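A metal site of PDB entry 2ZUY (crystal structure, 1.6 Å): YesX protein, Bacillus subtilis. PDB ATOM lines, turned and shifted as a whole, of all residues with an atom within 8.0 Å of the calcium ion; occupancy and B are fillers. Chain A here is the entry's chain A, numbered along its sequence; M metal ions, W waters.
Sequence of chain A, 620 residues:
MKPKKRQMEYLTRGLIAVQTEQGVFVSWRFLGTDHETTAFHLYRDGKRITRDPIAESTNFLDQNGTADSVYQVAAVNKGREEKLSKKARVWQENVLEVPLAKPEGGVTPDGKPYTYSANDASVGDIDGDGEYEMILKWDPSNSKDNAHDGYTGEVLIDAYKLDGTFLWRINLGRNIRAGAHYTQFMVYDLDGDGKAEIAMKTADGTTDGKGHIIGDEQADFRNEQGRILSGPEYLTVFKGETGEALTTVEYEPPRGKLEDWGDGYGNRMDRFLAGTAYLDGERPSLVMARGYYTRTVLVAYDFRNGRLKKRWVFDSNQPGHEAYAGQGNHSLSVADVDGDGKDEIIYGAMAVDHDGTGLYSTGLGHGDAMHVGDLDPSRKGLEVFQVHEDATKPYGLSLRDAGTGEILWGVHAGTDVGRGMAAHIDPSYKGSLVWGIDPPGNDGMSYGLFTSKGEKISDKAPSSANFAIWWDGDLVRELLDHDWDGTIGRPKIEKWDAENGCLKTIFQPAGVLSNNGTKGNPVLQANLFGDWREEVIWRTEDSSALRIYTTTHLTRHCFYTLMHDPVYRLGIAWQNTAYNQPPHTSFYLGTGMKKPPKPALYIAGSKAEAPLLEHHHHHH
The guanidinium group of Arg 379 sits at hydrogen-bond distance from the backbone carbonyl oxygen of Leu 382. OD1 of Asp 376 lies within hydrogen-bond range of OG of Ser 378, 2.7 Å away. OE1 of Glu 383 lies close to N of Leu 375. The backbone NH (N) of Glu 383 lies within hydrogen-bond range of the backbone carbonyl oxygen (O) of Gly 373.
Five residues have an atom within 4 Å of the calcium ion: Asp 374, Asp 376, Arg 379, Gly 381 and Glu 383. The nearest printed residue that does not touch the calcium ion is Pro 377 (4.1 Å).
The calcium ion is bound by the backbone carbonyl oxygen (O) of Arg 379. The backbone carbonyl oxygen (O) of Gly 381 is bound to the calcium ion (2.3 Å). The calcium ion is bound by OD1 of Asp 374, 2.4 Å away. The backbone carbonyl oxygen (O) of Asp 376 binds the calcium ion (2.4 Å). The side-chain carboxylate (OE2) of Glu 383 binds the calcium ion, 2.5 Å away. The calcium ion is bound by water W1, 2.6 Å away. The calcium ion is bound by OE1 of Glu 383.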
ATOM      1  N   GLY A 373      21.830   2.296  14.575  1.00  0.00           N
ATOM      2  CA  GLY A 373      22.366   1.379  13.566  1.00  0.00           C
ATOM      3  C   GLY A 373      23.502   0.592  14.160  1.00  0.00           C
ATOM      4  O   GLY A 373      23.710   0.608  15.380  1.00  0.00           O
ATOM      5  N   ASP A 374      24.232  -0.110  13.307  1.00  0.00           N
ATOM      6  CA  ASP A 374      25.416  -0.791  13.800  1.00  0.00           C
ATOM      7  C   ASP A 374      26.595   0.177  13.730  1.00  0.00           C
ATOM      8  O   ASP A 374      27.359   0.181  12.774  1.00  0.00           O
ATOM      9  CB  ASP A 374      25.701  -2.082  13.038  1.00  0.00           C
ATOM     10  CG  ASP A 374      26.751  -2.939  13.740  1.00  0.00           C
ATOM     11  OD1 ASP A 374      27.219  -2.513  14.821  1.00  0.00           O
ATOM     12  OD2 ASP A 374      27.082  -4.032  13.243  1.00  0.00           O
ATOM     13  N   LEU A 375      26.703   1.013  14.762  1.00  0.00           N
ATOM     14  CA  LEU A 375      27.693   2.089  14.793  1.00  0.00           C
ATOM     15  C   LEU A 375      29.072   1.592  15.198  1.00  0.00           C
ATOM     16  O   LEU A 375      30.085   2.163  14.797  1.00  0.00           O
ATOM     17  CB  LEU A 375      27.213   3.207  15.729  1.00  0.00           C
ATOM     18  CG  LEU A 375      25.759   3.664  15.527  1.00  0.00           C
ATOM     19  CD1 LEU A 375      25.437   4.821  16.460  1.00  0.00           C
ATOM     20  CD2 LEU A 375      25.454   4.052  14.074  1.00  0.00           C
ATOM     21  N   ASP A 376      29.095   0.534  16.009  1.00  0.00           N
ATOM     22  CA  ASP A 376      30.332  -0.120  16.429  1.00  0.00           C
ATOM     23  C   ASP A 376      30.199  -1.606  16.089  1.00  0.00           C
ATOM     24  O   ASP A 376      29.661  -2.380  16.896  1.00  0.00           O
ATOM     25  CB  ASP A 376      30.572   0.070  17.928  1.00  0.00           C
ATOM     26  CG  ASP A 376      31.815  -0.669  18.445  1.00  0.00           C
ATOM     27  OD1 ASP A 376      32.515  -1.320  17.633  1.00  0.00           O
ATOM     28  OD2 ASP A 376      32.089  -0.589  19.662  1.00  0.00           O
ATOM     29  N   PRO A 377      30.622  -2.004  14.882  1.00  0.00           N
ATOM     30  CA  PRO A 377      30.477  -3.413  14.448  1.00  0.00           C
ATOM     31  C   PRO A 377      31.309  -4.434  15.245  1.00  0.00           C
ATOM     32  O   PRO A 377      31.107  -5.641  15.067  1.00  0.00           O
ATOM     33  CB  PRO A 377      30.917  -3.391  12.978  1.00  0.00           C
ATOM     34  CG  PRO A 377      31.649  -2.105  12.795  1.00  0.00           C
ATOM     35  CD  PRO A 377      31.183  -1.150  13.817  1.00  0.00           C
ATOM     36  N   SER A 378      32.196  -3.969  16.107  1.00  0.00           N
ATOM     37  CA  SER A 378      33.013  -4.874  16.937  1.00  0.00           C
ATOM     38  C   SER A 378      32.231  -5.317  18.177  1.00  0.00           C
ATOM     39  O   SER A 378      32.634  -6.261  18.869  1.00  0.00           O
ATOM     40  CB  SER A 378      34.333  -4.208  17.346  1.00  0.00           C
ATOM     41  OG  SER A 378      34.139  -3.307  18.419  1.00  0.00           O
ATOM     42  N   ARG A 379      31.129  -4.622  18.433  1.00  0.00           N
ATOM     43  CA  ARG A 379      30.283  -4.849  19.580  1.00  0.00           C
ATOM     44  C   ARG A 379      28.937  -5.416  19.114  1.00  0.00           C
ATOM     45  O   ARG A 379      28.251  -4.792  18.297  1.00  0.00           O
ATOM     46  CB  ARG A 379      30.076  -3.526  20.314  1.00  0.00           C
ATOM     47  CG  ARG A 379      29.846  -3.624  21.807  1.00  0.00           C
ATOM     48  CD  ARG A 379      29.174  -2.363  22.308  1.00  0.00           C
ATOM     49  NE  ARG A 379      27.823  -2.265  21.764  1.00  0.00           N
ATOM     50  CZ  ARG A 379      26.730  -2.676  22.390  1.00  0.00           C
ATOM     51  NH1 ARG A 379      26.809  -3.206  23.616  1.00  0.00           N
ATOM     52  NH2 ARG A 379      25.553  -2.552  21.796  1.00  0.00           N
ATOM     53  N   LYS A 380      28.573  -6.597  19.621  1.00  0.00           N
ATOM     54  CA  LYS A 380      27.332  -7.256  19.237  1.00  0.00           C
ATOM     55  C   LYS A 380      26.110  -6.348  19.458  1.00  0.00           C
ATOM     56  O   LYS A 380      25.975  -5.718  20.507  1.00  0.00           O
ATOM     57  CB  LYS A 380      27.155  -8.569  20.019  1.00  0.00           C
ATOM     58  CG  LYS A 380      25.980  -9.434  19.574  1.00  0.00           C
ATOM     59  CD  LYS A 380      26.315 -10.296  18.355  1.00  0.00           C
ATOM     60  CE  LYS A 380      27.068 -11.571  18.739  1.00  0.00           C
ATOM     61  NZ  LYS A 380      26.235 -12.551  19.501  1.00  0.00           N
ATOM     62  N   GLY A 381      25.245  -6.300  18.445  1.00  0.00           N
ATOM     63  CA  GLY A 381      24.004  -5.542  18.513  1.00  0.00           C
ATOM     64  C   GLY A 381      24.091  -4.158  17.897  1.00  0.00           C
ATOM     65  O   GLY A 381      25.118  -3.775  17.351  1.00  0.00           O
ATOM     66  N   LEU A 382      22.991  -3.413  18.008  1.00  0.00           N
ATOM     67  CA  LEU A 382      22.933  -2.044  17.523  1.00  0.00           C
ATOM     68  C   LEU A 382      23.326  -1.065  18.628  1.00  0.00           C
ATOM     69  O   LEU A 382      23.329  -1.410  19.809  1.00  0.00           O
ATOM     70  CB  LEU A 382      21.527  -1.718  17.003  1.00  0.00           C
ATOM     71  CG  LEU A 382      21.003  -2.584  15.858  1.00  0.00           C
ATOM     72  CD1 LEU A 382      19.642  -2.063  15.402  1.00  0.00           C
ATOM     73  CD2 LEU A 382      21.986  -2.614  14.680  1.00  0.00           C
ATOM     74  N   GLU A 383      23.655   0.161  18.223  1.00  0.00           N
ATOM     75  CA  GLU A 383      24.002   1.221  19.148  1.00  0.00           C
ATOM     76  C   GLU A 383      23.165   2.436  18.824  1.00  0.00           C
ATOM     77  O   GLU A 383      22.679   2.575  17.698  1.00  0.00           O
ATOM     78  CB  GLU A 383      25.493   1.563  19.027  1.00  0.00           C
ATOM     79  CG  GLU A 383      26.445   0.497  19.599  1.00  0.00           C
ATOM     80  CD  GLU A 383      26.739  -0.670  18.646  1.00  0.00           C
ATOM     81  OE1 GLU A 383      26.762  -0.486  17.402  1.00  0.00           O
ATOM     82  OE2 GLU A 383      26.945  -1.795  19.155  1.00  0.00           O
ATOM     83  N   ARG A 400      25.260   4.608  23.190  1.00  0.00           N
ATOM     84  CA  ARG A 400      24.757   3.545  24.067  1.00  0.00           C
ATOM     85  C   ARG A 400      24.424   2.250  23.344  1.00  0.00           C
ATOM     86  O   ARG A 400      24.234   2.219  22.122  1.00  0.00           O
ATOM     87  CB  ARG A 400      23.520   4.042  24.824  1.00  0.00           C
ATOM     88  CG  ARG A 400      22.254   4.193  23.968  1.00  0.00           C
ATOM     89  CD  ARG A 400      21.156   4.800  24.808  1.00  0.00           C
ATOM     90  NE  ARG A 400      19.826   4.757  24.208  1.00  0.00           N
ATOM     91  CZ  ARG A 400      19.201   5.817  23.688  1.00  0.00           C
ATOM     92  NH1 ARG A 400      19.803   7.008  23.633  1.00  0.00           N
ATOM     93  NH2 ARG A 400      17.968   5.689  23.214  1.00  0.00           N
ATOM     94  N   ALA A 402      21.918  -0.163  22.139  1.00  0.00           N
ATOM     95  CA  ALA A 402      20.543   0.140  21.726  1.00  0.00           C
ATOM     96  C   ALA A 402      19.482  -0.650  22.476  1.00  0.00           C
ATOM     97  O   ALA A 402      18.373  -0.159  22.703  1.00  0.00           O
ATOM     98  CB  ALA A 402      20.379  -0.050  20.216  1.00  0.00           C
ATOM     99  N   LEU A 408      27.663   3.649  26.937  1.00  0.00           N
ATOM    100  CA  LEU A 408      29.014   3.142  26.715  1.00  0.00           C
ATOM    101  C   LEU A 408      30.032   4.251  26.939  1.00  0.00           C
ATOM    102  O   LEU A 408      31.070   4.038  27.562  1.00  0.00           O
ATOM    103  CB  LEU A 408      29.124   2.525  25.315  1.00  0.00           C
ATOM    104  CG  LEU A 408      28.163   1.327  25.133  1.00  0.00           C
ATOM    105  CD1 LEU A 408      28.079   0.937  23.674  1.00  0.00           C
ATOM    106  CD2 LEU A 408      28.571   0.133  25.992  1.00  0.00           C
ATOM    107  N   SER A 452      33.173   5.542  17.287  1.00  0.00           N
ATOM    108  CA  SER A 452      32.034   5.041  18.075  1.00  0.00           C
ATOM    109  C   SER A 452      32.465   4.343  19.373  1.00  0.00           C
ATOM    110  O   SER A 452      31.644   4.064  20.233  1.00  0.00           O
ATOM    111  CB  SER A 452      31.136   4.124  17.239  1.00  0.00           C
ATOM    112  OG  SER A 452      31.851   3.010  16.721  1.00  0.00           O
ATOM    113  N   TYR A 588      25.921  -3.329   9.406  1.00  0.00           N
ATOM    114  CA  TYR A 588      27.027  -2.423   9.188  1.00  0.00           C
ATOM    115  C   TYR A 588      27.370  -2.389   7.708  1.00  0.00           C
ATOM    116  O   TYR A 588      27.781  -3.397   7.135  1.00  0.00           O
ATOM    117  CB  TYR A 588      28.256  -2.819  10.013  1.00  0.00           C
ATOM    118  CG  TYR A 588      29.497  -2.049   9.626  1.00  0.00           C
ATOM    119  CD1 TYR A 588      29.526  -0.653   9.675  1.00  0.00           C
ATOM    120  CD2 TYR A 588      30.649  -2.717   9.192  1.00  0.00           C
ATOM    121  CE1 TYR A 588      30.676   0.052   9.305  1.00  0.00           C
ATOM    122  CE2 TYR A 588      31.792  -2.019   8.823  1.00  0.00           C
ATOM    123  CZ  TYR A 588      31.798  -0.630   8.873  1.00  0.00           C
ATOM    124  OH  TYR A 588      32.935   0.060   8.507  1.00  0.00           O
HETATM  125 CA    CA M   1      27.341  -3.097  17.101  1.00  0.00          CA
HETATM  126  O   HOH W   1      27.553  -5.188  15.627  1.00  0.00           O
